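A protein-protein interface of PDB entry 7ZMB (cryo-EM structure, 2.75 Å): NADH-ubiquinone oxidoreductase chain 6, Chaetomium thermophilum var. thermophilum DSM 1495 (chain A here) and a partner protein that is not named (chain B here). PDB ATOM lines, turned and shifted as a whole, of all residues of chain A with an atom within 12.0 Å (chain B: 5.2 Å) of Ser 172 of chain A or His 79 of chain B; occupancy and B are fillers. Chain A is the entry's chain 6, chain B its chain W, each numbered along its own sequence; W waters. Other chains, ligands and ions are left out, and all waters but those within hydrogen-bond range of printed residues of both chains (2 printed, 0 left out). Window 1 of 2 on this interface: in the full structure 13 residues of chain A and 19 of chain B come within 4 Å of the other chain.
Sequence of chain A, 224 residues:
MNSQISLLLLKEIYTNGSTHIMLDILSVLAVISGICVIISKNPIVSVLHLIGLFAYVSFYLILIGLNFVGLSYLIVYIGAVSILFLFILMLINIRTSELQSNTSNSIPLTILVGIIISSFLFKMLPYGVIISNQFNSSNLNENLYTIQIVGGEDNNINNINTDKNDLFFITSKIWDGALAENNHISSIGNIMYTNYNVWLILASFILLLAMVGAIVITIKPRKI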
ATOM      1  N   LEU A   7     -23.110 -29.237  -6.608  1.00  0.00           N
ATOM      2  CA  LEU A   7     -24.360 -29.190  -7.424  1.00  0.00           C
ATOM      3  C   LEU A   7     -25.557 -29.047  -6.500  1.00  0.00           C
ATOM      4  O   LEU A   7     -25.743 -29.934  -5.650  1.00  0.00           O
ATOM      5  CB  LEU A   7     -24.520 -30.408  -8.344  1.00  0.00           C
ATOM      6  CG  LEU A   7     -23.923 -30.301  -9.752  1.00  0.00           C
ATOM      7  CD1 LEU A   7     -24.299 -31.518 -10.582  1.00  0.00           C
ATOM      8  CD2 LEU A   7     -24.377 -29.035 -10.455  1.00  0.00           C
ATOM      9  N   GLU A  12     -38.050 -24.394  -6.659  1.00  0.00           N
ATOM     10  CA  GLU A  12     -38.357 -22.984  -7.007  1.00  0.00           C
ATOM     11  C   GLU A  12     -39.530 -22.486  -6.153  1.00  0.00           C
ATOM     12  O   GLU A  12     -40.596 -23.108  -6.203  1.00  0.00           O
ATOM     13  CB  GLU A  12     -38.705 -22.928  -8.489  1.00  0.00           C
ATOM     14  CG  GLU A  12     -38.381 -21.600  -9.141  1.00  0.00           C
ATOM     15  CD  GLU A  12     -38.466 -21.652 -10.655  1.00  0.00           C
ATOM     16  OE1 GLU A  12     -38.476 -22.770 -11.201  1.00  0.00           O
ATOM     17  OE2 GLU A  12     -38.538 -20.582 -11.278  1.00  0.00           O
ATOM     18  N   THR A  15     -42.293 -18.072  -9.249  1.00  0.00           N
ATOM     19  CA  THR A  15     -41.779 -18.049 -10.612  1.00  0.00           C
ATOM     20  C   THR A  15     -41.640 -19.447 -11.207  1.00  0.00           C
ATOM     21  O   THR A  15     -41.065 -19.603 -12.290  1.00  0.00           O
ATOM     22  CB  THR A  15     -40.434 -17.312 -10.691  1.00  0.00           C
ATOM     23  OG1 THR A  15     -39.457 -17.985  -9.891  1.00  0.00           O
ATOM     24  CG2 THR A  15     -40.584 -15.907 -10.157  1.00  0.00           C
ATOM     25  N   PHE A 168     -33.197 -34.125 -17.144  1.00  0.00           N
ATOM     26  CA  PHE A 168     -33.876 -32.862 -16.772  1.00  0.00           C
ATOM     27  C   PHE A 168     -33.432 -31.791 -17.764  1.00  0.00           C
ATOM     28  O   PHE A 168     -32.217 -31.605 -17.960  1.00  0.00           O
ATOM     29  CB  PHE A 168     -33.603 -32.501 -15.313  1.00  0.00           C
ATOM     30  CG  PHE A 168     -34.201 -33.455 -14.310  1.00  0.00           C
ATOM     31  CD1 PHE A 168     -35.520 -33.327 -13.906  1.00  0.00           C
ATOM     32  CD2 PHE A 168     -33.449 -34.487 -13.773  1.00  0.00           C
ATOM     33  CE1 PHE A 168     -36.072 -34.205 -12.988  1.00  0.00           C
ATOM     34  CE2 PHE A 168     -34.000 -35.365 -12.854  1.00  0.00           C
ATOM     35  CZ  PHE A 168     -35.310 -35.221 -12.462  1.00  0.00           C
ATOM     36  N   PHE A 169     -34.406 -31.162 -18.417  1.00  0.00           N
ATOM     37  CA  PHE A 169     -34.082 -30.057 -19.346  1.00  0.00           C
ATOM     38  C   PHE A 169     -33.627 -28.864 -18.511  1.00  0.00           C
ATOM     39  O   PHE A 169     -34.231 -28.600 -17.465  1.00  0.00           O
ATOM     40  CB  PHE A 169     -35.276 -29.756 -20.255  1.00  0.00           C
ATOM     41  CG  PHE A 169     -35.750 -30.893 -21.122  1.00  0.00           C
ATOM     42  CD1 PHE A 169     -35.199 -31.107 -22.374  1.00  0.00           C
ATOM     43  CD2 PHE A 169     -36.764 -31.734 -20.698  1.00  0.00           C
ATOM     44  CE1 PHE A 169     -35.649 -32.140 -23.180  1.00  0.00           C
ATOM     45  CE2 PHE A 169     -37.206 -32.773 -21.501  1.00  0.00           C
ATOM     46  CZ  PHE A 169     -36.647 -32.975 -22.739  1.00  0.00           C
ATOM     47  N   ILE A 170     -32.572 -28.188 -18.958  1.00  0.00           N
ATOM     48  CA  ILE A 170     -32.031 -27.021 -18.208  1.00  0.00           C
ATOM     49  C   ILE A 170     -32.217 -25.763 -19.058  1.00  0.00           C
ATOM     50  O   ILE A 170     -31.923 -25.810 -20.260  1.00  0.00           O
ATOM     51  CB  ILE A 170     -30.572 -27.275 -17.782  1.00  0.00           C
ATOM     52  CG1 ILE A 170     -30.079 -26.241 -16.769  1.00  0.00           C
ATOM     53  CG2 ILE A 170     -29.634 -27.424 -18.968  1.00  0.00           C
ATOM     54  CD1 ILE A 170     -30.544 -26.510 -15.364  1.00  0.00           C
ATOM     55  N   THR A 171     -32.748 -24.699 -18.459  1.00  0.00           N
ATOM     56  CA  THR A 171     -32.936 -23.421 -19.195  1.00  0.00           C
ATOM     57  C   THR A 171     -32.259 -22.271 -18.444  1.00  0.00           C
ATOM     58  O   THR A 171     -32.180 -22.336 -17.218  1.00  0.00           O
ATOM     59  CB  THR A 171     -34.413 -23.145 -19.497  1.00  0.00           C
ATOM     60  OG1 THR A 171     -35.092 -22.814 -18.285  1.00  0.00           O
ATOM     61  CG2 THR A 171     -35.103 -24.296 -20.189  1.00  0.00           C
ATOM     62  N   SER A 172     -31.723 -21.300 -19.177  1.00  0.00           N
ATOM     63  CA  SER A 172     -31.106 -20.104 -18.554  1.00  0.00           C
ATOM     64  C   SER A 172     -31.647 -18.853 -19.251  1.00  0.00           C
ATOM     65  O   SER A 172     -32.667 -18.969 -19.938  1.00  0.00           O
ATOM     66  CB  SER A 172     -29.615 -20.163 -18.630  1.00  0.00           C
ATOM     67  OG  SER A 172     -29.187 -20.125 -19.977  1.00  0.00           O
ATOM     68  N   LYS A 173     -30.972 -17.717 -19.121  1.00  0.00           N
ATOM     69  CA  LYS A 173     -31.515 -16.466 -19.694  1.00  0.00           C
ATOM     70  C   LYS A 173     -30.510 -15.794 -20.627  1.00  0.00           C
ATOM     71  O   LYS A 173     -29.314 -16.021 -20.440  1.00  0.00           O
ATOM     72  CB  LYS A 173     -31.895 -15.553 -18.529  1.00  0.00           C
ATOM     73  CG  LYS A 173     -30.737 -14.984 -17.724  1.00  0.00           C
ATOM     74  CD  LYS A 173     -31.171 -14.029 -16.645  1.00  0.00           C
ATOM     75  CE  LYS A 173     -32.019 -14.675 -15.573  1.00  0.00           C
ATOM     76  NZ  LYS A 173     -32.385 -13.700 -14.518  1.00  0.00           N
ATOM     77  N   ILE A 174     -30.982 -15.051 -21.629  1.00  0.00           N
ATOM     78  CA  ILE A 174     -30.075 -14.211 -22.465  1.00  0.00           C
ATOM     79  C   ILE A 174     -30.686 -12.815 -22.438  1.00  0.00           C
ATOM     80  O   ILE A 174     -31.849 -12.700 -22.043  1.00  0.00           O
ATOM     81  CB  ILE A 174     -29.865 -14.709 -23.913  1.00  0.00           C
ATOM     82  CG1 ILE A 174     -31.186 -14.948 -24.648  1.00  0.00           C
ATOM     83  CG2 ILE A 174     -28.949 -15.922 -23.961  1.00  0.00           C
ATOM     84  CD1 ILE A 174     -31.013 -15.234 -26.120  1.00  0.00           C
ATOM     85  N   TRP A 175     -29.910 -11.798 -22.786  1.00  0.00           N
ATOM     86  CA  TRP A 175     -30.395 -10.399 -22.784  1.00  0.00           C
ATOM     87  C   TRP A 175     -30.483  -9.859 -24.213  1.00  0.00           C
ATOM     88  O   TRP A 175     -31.403  -9.082 -24.486  1.00  0.00           O
ATOM     89  CB  TRP A 175     -29.458  -9.584 -21.893  1.00  0.00           C
ATOM     90  CG  TRP A 175     -29.479 -10.069 -20.476  1.00  0.00           C
ATOM     91  CD1 TRP A 175     -28.587 -10.908 -19.879  1.00  0.00           C
ATOM     92  CD2 TRP A 175     -30.472  -9.768 -19.478  1.00  0.00           C
ATOM     93  NE1 TRP A 175     -28.943 -11.136 -18.580  1.00  0.00           N
ATOM     94  CE2 TRP A 175     -30.095 -10.450 -18.303  1.00  0.00           C
ATOM     95  CE3 TRP A 175     -31.629  -8.982 -19.457  1.00  0.00           C
ATOM     96  CZ2 TRP A 175     -30.834 -10.372 -17.125  1.00  0.00           C
ATOM     97  CZ3 TRP A 175     -32.361  -8.907 -18.294  1.00  0.00           C
ATOM     98  CH2 TRP A 175     -31.964  -9.588 -17.144  1.00  0.00           C
ATOM     99  N   ASP A 176     -29.577 -10.280 -25.090  1.00  0.00           N
ATOM    100  CA  ASP A 176     -29.551  -9.811 -26.502  1.00  0.00           C
ATOM    101  C   ASP A 176     -30.803 -10.310 -27.230  1.00  0.00           C
ATOM    102  O   ASP A 176     -31.324  -9.576 -28.071  1.00  0.00           O
ATOM    103  CB  ASP A 176     -28.251 -10.187 -27.209  1.00  0.00           C
ATOM    104  CG  ASP A 176     -26.991  -9.845 -26.438  1.00  0.00           C
ATOM    105  OD1 ASP A 176     -27.101  -9.513 -25.248  1.00  0.00           O
ATOM    106  OD2 ASP A 176     -25.905  -9.914 -27.036  1.00  0.00           O
ATOM    107  N   GLY A 177     -31.251 -11.521 -26.914  1.00  0.00           N
ATOM    108  CA  GLY A 177     -32.461 -12.093 -27.530  1.00  0.00           C
ATOM    109  C   GLY A 177     -33.714 -11.729 -26.767  1.00  0.00           C
ATOM    110  O   GLY A 177     -34.779 -12.221 -27.137  1.00  0.00           O
ATOM    111  N   ALA A 178     -33.579 -10.914 -25.724  1.00  0.00           N
ATOM    112  CA  ALA A 178     -34.749 -10.477 -24.931  1.00  0.00           C
ATOM    113  C   ALA A 178     -35.015  -8.980 -25.084  1.00  0.00           C
ATOM    114  O   ALA A 178     -35.862  -8.475 -24.326  1.00  0.00           O
ATOM    115  CB  ALA A 178     -34.544 -10.825 -23.487  1.00  0.00           C
ATOM    116  N   GLU A 181     -38.983  -9.082 -26.675  1.00  0.00           N
ATOM    117  CA  GLU A 181     -39.580 -10.428 -26.876  1.00  0.00           C
ATOM    118  C   GLU A 181     -40.986 -10.265 -27.457  1.00  0.00           C
ATOM    119  O   GLU A 181     -41.774  -9.495 -26.882  1.00  0.00           O
ATOM    120  CB  GLU A 181     -39.591 -11.247 -25.587  1.00  0.00           C
ATOM    121  CG  GLU A 181     -40.430 -12.508 -25.660  1.00  0.00           C
ATOM    122  CD  GLU A 181     -41.626 -12.516 -24.723  1.00  0.00           C
ATOM    123  OE1 GLU A 181     -41.634 -11.714 -23.771  1.00  0.00           O
ATOM    124  OE2 GLU A 181     -42.553 -13.316 -24.956  1.00  0.00           O
ATOM    125  N   GLU B  75     -23.810 -12.934 -17.789  1.00  0.00           N
ATOM    126  CA  GLU B  75     -24.407 -14.233 -18.185  1.00  0.00           C
ATOM    127  C   GLU B  75     -23.339 -15.122 -18.823  1.00  0.00           C
ATOM    128  O   GLU B  75     -23.338 -16.325 -18.548  1.00  0.00           O
ATOM    129  CB  GLU B  75     -25.612 -13.997 -19.095  1.00  0.00           C
ATOM    130  CG  GLU B  75     -26.502 -15.213 -19.230  1.00  0.00           C
ATOM    131  CD  GLU B  75     -27.094 -15.714 -17.924  1.00  0.00           C
ATOM    132  OE1 GLU B  75     -27.441 -14.872 -17.069  1.00  0.00           O
ATOM    133  OE2 GLU B  75     -27.204 -16.942 -17.763  1.00  0.00           O
ATOM    134  N   ASP B  76     -22.480 -14.542 -19.656  1.00  0.00           N
ATOM    135  CA  ASP B  76     -21.405 -15.307 -20.342  1.00  0.00           C
ATOM    136  C   ASP B  76     -20.399 -15.839 -19.324  1.00  0.00           C
ATOM    137  O   ASP B  76     -19.974 -16.982 -19.478  1.00  0.00           O
ATOM    138  CB  ASP B  76     -20.713 -14.471 -21.413  1.00  0.00           C
ATOM    139  CG  ASP B  76     -21.598 -14.123 -22.598  1.00  0.00           C
ATOM    140  OD1 ASP B  76     -22.819 -14.351 -22.514  1.00  0.00           O
ATOM    141  OD2 ASP B  76     -21.052 -13.635 -23.598  1.00  0.00           O
ATOM    142  N   ARG B  77     -20.061 -15.041 -18.311  1.00  0.00           N
ATOM    143  CA  ARG B  77     -19.123 -15.508 -17.264  1.00  0.00           C
ATOM    144  C   ARG B  77     -19.745 -16.706 -16.550  1.00  0.00           C
ATOM    145  O   ARG B  77     -19.019 -17.668 -16.302  1.00  0.00           O
ATOM    146  CB  ARG B  77     -18.718 -14.357 -16.341  1.00  0.00           C
ATOM    147  CG  ARG B  77     -17.629 -13.460 -16.907  1.00  0.00           C
ATOM    148  CD  ARG B  77     -17.248 -12.412 -15.885  1.00  0.00           C
ATOM    149  NE  ARG B  77     -18.316 -11.457 -15.650  1.00  0.00           N
ATOM    150  CZ  ARG B  77     -18.383 -10.256 -16.206  1.00  0.00           C
ATOM    151  NH1 ARG B  77     -17.432  -9.853 -17.029  1.00  0.00           N
ATOM    152  NH2 ARG B  77     -19.394  -9.457 -15.929  1.00  0.00           N
ATOM    153  N   ASP B  78     -21.045 -16.651 -16.268  1.00  0.00           N
ATOM    154  CA  ASP B  78     -21.767 -17.788 -15.637  1.00  0.00           C
ATOM    155  C   ASP B  78     -21.765 -19.001 -16.575  1.00  0.00           C
ATOM    156  O   ASP B  78     -21.524 -20.110 -16.082  1.00  0.00           O
ATOM    157  CB  ASP B  78     -23.194 -17.354 -15.301  1.00  0.00           C
ATOM    158  CG  ASP B  78     -24.053 -18.445 -14.693  1.00  0.00           C
ATOM    159  OD1 ASP B  78     -23.744 -18.866 -13.566  1.00  0.00           O
ATOM    160  OD2 ASP B  78     -25.027 -18.856 -15.352  1.00  0.00           O
ATOM    161  N   HIS B  79     -22.006 -18.792 -17.871  1.00  0.00           N
ATOM    162  CA  HIS B  79     -22.075 -19.898 -18.863  1.00  0.00           C
ATOM    163  C   HIS B  79     -20.714 -20.566 -19.008  1.00  0.00           C
ATOM    164  O   HIS B  79     -20.683 -21.801 -19.115  1.00  0.00           O
ATOM    165  CB  HIS B  79     -22.667 -19.403 -20.190  1.00  0.00           C
ATOM    166  CG  HIS B  79     -24.156 -19.408 -20.189  1.00  0.00           C
ATOM    167  ND1 HIS B  79     -24.889 -20.301 -20.936  1.00  0.00           N
ATOM    168  CD2 HIS B  79     -25.050 -18.658 -19.511  1.00  0.00           C
ATOM    169  CE1 HIS B  79     -26.170 -20.086 -20.737  1.00  0.00           C
ATOM    170  NE2 HIS B  79     -26.295 -19.085 -19.866  1.00  0.00           N
ATOM    171  N   VAL B  80     -19.642 -19.775 -18.970  1.00  0.00           N
ATOM    172  CA  VAL B  80     -18.277 -20.317 -19.180  1.00  0.00           C
ATOM    173  C   VAL B  80     -17.861 -20.938 -17.855  1.00  0.00           C
ATOM    174  O   VAL B  80     -17.288 -22.036 -17.883  1.00  0.00           O
ATOM    175  CB  VAL B  80     -17.323 -19.175 -19.591  1.00  0.00           C
ATOM    176  CG1 VAL B  80     -15.855 -19.542 -19.451  1.00  0.00           C
ATOM    177  CG2 VAL B  80     -17.623 -18.648 -20.984  1.00  0.00           C
ATOM    178  N   ARG B  81     -18.238 -20.314 -16.739  1.00  0.00           N
ATOM    179  CA  ARG B  81     -17.966 -20.932 -15.414  1.00  0.00           C
ATOM    180  C   ARG B  81     -18.623 -22.306 -15.287  1.00  0.00           C
ATOM    181  O   ARG B  81     -17.970 -23.195 -14.741  1.00  0.00           O
ATOM    182  CB  ARG B  81     -18.488 -20.028 -14.304  1.00  0.00           C
ATOM    183  CG  ARG B  81     -17.991 -20.377 -12.911  1.00  0.00           C
ATOM    184  CD  ARG B  81     -18.573 -19.431 -11.883  1.00  0.00           C
ATOM    185  NE  ARG B  81     -20.022 -19.327 -11.969  1.00  0.00           N
ATOM    186  CZ  ARG B  81     -20.869 -20.224 -11.487  1.00  0.00           C
ATOM    187  NH1 ARG B  81     -22.171 -20.045 -11.605  1.00  0.00           N
ATOM    188  NH2 ARG B  81     -20.409 -21.312 -10.902  1.00  0.00           N
ATOM    189  N   ARG B  82     -19.814 -22.515 -15.854  1.00  0.00           N
ATOM    190  CA  ARG B  82     -20.439 -23.846 -15.649  1.00  0.00           C
ATOM    191  C   ARG B  82     -19.999 -24.838 -16.711  1.00  0.00           C
ATOM    192  O   ARG B  82     -20.008 -26.031 -16.412  1.00  0.00           O
ATOM    193  CB  ARG B  82     -21.961 -23.720 -15.514  1.00  0.00           C
ATOM    194  CG  ARG B  82     -22.395 -22.802 -14.380  1.00  0.00           C
ATOM    195  CD  ARG B  82     -23.883 -22.694 -14.122  1.00  0.00           C
ATOM    196  NE  ARG B  82     -24.480 -23.963 -13.744  1.00  0.00           N
ATOM    197  CZ  ARG B  82     -25.628 -24.094 -13.095  1.00  0.00           C
ATOM    198  NH1 ARG B  82     -26.087 -25.298 -12.806  1.00  0.00           N
ATOM    199  NH2 ARG B  82     -26.307 -23.025 -12.727  1.00  0.00           N
ATOM    200  N   TYR B  83     -19.726 -24.357 -17.924  1.00  0.00           N
ATOM    201  CA  TYR B  83     -19.235 -25.270 -18.984  1.00  0.00           C
ATOM    202  C   TYR B  83     -17.891 -25.852 -18.561  1.00  0.00           C
ATOM    203  O   TYR B  83     -17.747 -27.073 -18.615  1.00  0.00           O
ATOM    204  CB  TYR B  83     -19.065 -24.520 -20.309  1.00  0.00           C
ATOM    205  CG  TYR B  83     -18.469 -25.346 -21.418  1.00  0.00           C
ATOM    206  CD1 TYR B  83     -19.265 -26.141 -22.220  1.00  0.00           C
ATOM    207  CD2 TYR B  83     -17.104 -25.348 -21.657  1.00  0.00           C
ATOM    208  CE1 TYR B  83     -18.726 -26.909 -23.236  1.00  0.00           C
ATOM    209  CE2 TYR B  83     -16.548 -26.109 -22.669  1.00  0.00           C
ATOM    210  CZ  TYR B  83     -17.364 -26.892 -23.462  1.00  0.00           C
ATOM    211  OH  TYR B  83     -16.828 -27.648 -24.465  1.00  0.00           O
ATOM    212  N   LEU B  84     -16.974 -25.005 -18.095  1.00  0.00           N
ATOM    213  CA  LEU B  84     -15.615 -25.448 -17.701  1.00  0.00           C
ATOM    214  C   LEU B  84     -15.759 -26.382 -16.516  1.00  0.00           C
ATOM    215  O   LEU B  84     -15.016 -27.373 -16.458  1.00  0.00           O
ATOM    216  CB  LEU B  84     -14.760 -24.221 -17.365  1.00  0.00           C
ATOM    217  CG  LEU B  84     -14.389 -23.346 -18.560  1.00  0.00           C
ATOM    218  CD1 LEU B  84     -13.583 -22.142 -18.114  1.00  0.00           C
ATOM    219  CD2 LEU B  84     -13.620 -24.144 -19.597  1.00  0.00           C
ATOM    220  N   TYR B 106     -19.686 -23.092 -28.703  1.00  0.00           N
ATOM    221  CA  TYR B 106     -20.382 -23.363 -27.428  1.00  0.00           C
ATOM    222  C   TYR B 106     -21.875 -23.495 -27.699  1.00  0.00           C
ATOM    223  O   TYR B 106     -22.439 -22.649 -28.412  1.00  0.00           O
ATOM    224  CB  TYR B 106     -20.180 -22.224 -26.433  1.00  0.00           C
ATOM    225  CG  TYR B 106     -21.040 -22.347 -25.202  1.00  0.00           C
ATOM    226  CD1 TYR B 106     -20.854 -23.390 -24.311  1.00  0.00           C
ATOM    227  CD2 TYR B 106     -22.059 -21.447 -24.945  1.00  0.00           C
ATOM    228  CE1 TYR B 106     -21.648 -23.531 -23.189  1.00  0.00           C
ATOM    229  CE2 TYR B 106     -22.861 -21.571 -23.824  1.00  0.00           C
ATOM    230  CZ  TYR B 106     -22.653 -22.617 -22.943  1.00  0.00           C
ATOM    231  OH  TYR B 106     -23.427 -22.753 -21.831  1.00  0.00           O
ATOM    232  N   ARG B 108     -25.560 -23.732 -25.684  1.00  0.00           N
ATOM    233  CA  ARG B 108     -26.290 -23.631 -24.396  1.00  0.00           C
ATOM    234  C   ARG B 108     -26.884 -24.999 -23.997  1.00  0.00           C
ATOM    235  O   ARG B 108     -27.820 -25.433 -24.692  1.00  0.00           O
ATOM    236  CB  ARG B 108     -27.274 -22.462 -24.477  1.00  0.00           C
ATOM    237  CG  ARG B 108     -26.614 -21.121 -24.208  1.00  0.00           C
ATOM    238  CD  ARG B 108     -27.437 -19.979 -24.747  1.00  0.00           C
ATOM    239  NE  ARG B 108     -26.814 -18.691 -24.502  1.00  0.00           N
ATOM    240  CZ  ARG B 108     -26.038 -18.056 -25.370  1.00  0.00           C
ATOM    241  NH1 ARG B 108     -25.525 -16.880 -25.063  1.00  0.00           N
ATOM    242  NH2 ARG B 108     -25.781 -18.599 -26.546  1.00  0.00           N
ATOM    243  N   PRO B 109     -26.450 -25.677 -22.895  1.00  0.00           N
ATOM    244  CA  PRO B 109     -26.923 -27.030 -22.548  1.00  0.00           C
ATOM    245  C   PRO B 109     -28.436 -27.284 -22.577  1.00  0.00           C
ATOM    246  O   PRO B 109     -29.152 -26.511 -22.001  1.00  0.00           O
ATOM    247  CB  PRO B 109     -26.462 -27.178 -21.095  1.00  0.00           C
ATOM    248  CG  PRO B 109     -25.237 -26.311 -20.998  1.00  0.00           C
ATOM    249  CD  PRO B 109     -25.553 -25.124 -21.879  1.00  0.00           C
HETATM  250  O   HOH W   1     -29.822 -18.027 -16.171  1.00  0.00           O
HETATM  251  O   HOH W   2     -28.932 -18.794 -22.272  1.00  0.00           O
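Water W2 lies within hydrogen-bond range of the side-chain hydroxyl of Ser 172 of chain A (2.7 Å), the guanidinium group of Arg 108 of chain B (3.1 Å) and the backbone carbonyl oxygen of Lys 173 of chain A (3.3 Å). Water W1 lies within hydrogen-bond range of N of Lys 173 of chain A and OE2 of Glu 75 of chain B.
NE2 of His 79 of chain B is in hydrogen-bond range of OG of Ser 172 of chain A, 3.1 Å away. O of Ile 170 of chain A sits close to O of Pro 109 of chain B, 3.3 Å away.
Of the 13 printed residues of chain B, 4 touch a printed residue of chain A. Printed residues of chain B that touch a printed residue of chain A: Glu 75, His 79, Arg 108 and Pro 109. Of the 15 printed residues of chain A, 4 touch a printed residue of chain B. Hydrophobic or aromatic side chains of chain A within 4 Å of the printed part of chain B: Ile 170 and Ile 174. Among the printed residues, no Asp or Glu carboxylate lies within 4 Å of a Lys or Arg side-chain nitrogen of the other chain.
Glu 75 of chain B touches Lys 173 of chain A (CG to O, 3.2 Å). CG2 of Ile 174 of chain A touches NE of Arg 108 of chain B, at 3.5 Å.
Of the printed residues of chain B, Ser 172 of chain A touches His 79 (3.1 Å). His 79 of chain B touches just one residue of chain A: Ser 172 (3.1 Å). Of the printed residues of chain A, Glu 75 of chain B touches Lys 173 (3.2 Å). No residue of chain A comes within 4 Å of Asp 78 of chain B. No residue of chain A comes within 4 Å of Val 80 of chain B. No residue of chain A comes within 4 Å of Arg 81 of chain B. Of chain A, only Ile 174 comes within 4 Å of Arg 108 of chain B. Of chain A, only Ile 170 (3.2 Å) comes within 4 Å of Pro 109 of chain B. Of the printed residues of chain B, Ile 170 of chain A touches Pro 109. Printed residues of chain B within 4 Å of Ile 174 of chain A: Arg 108. Of the printed residues of chain B, Lys 173 of chain A touches Glu 75. Phe 169 of chain A touches none of the printed residues of chain B. The nearest residue of chain B that does not touch Ser 172 of chain A is Glu 75 of chain B (4.1 Å). The nearest residue of chain A that does not touch His 79 of chain B is Lys 173 of chain A (4.3 Å). The nearest printed residue of chain B that does not touch Ile 170 of chain A is Arg 82 of chain B (5.3 Å).
OE2 of Glu 75 of chain B sits at hydrogen-bond distance from NE2 of His 79 of chain B, 3.1 Å away. A ring nitrogen (ND1) of His 79 of chain B sits at hydrogen-bond distance from the side-chain hydroxyl (OH) of Tyr 106 of chain B (3.0 Å).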
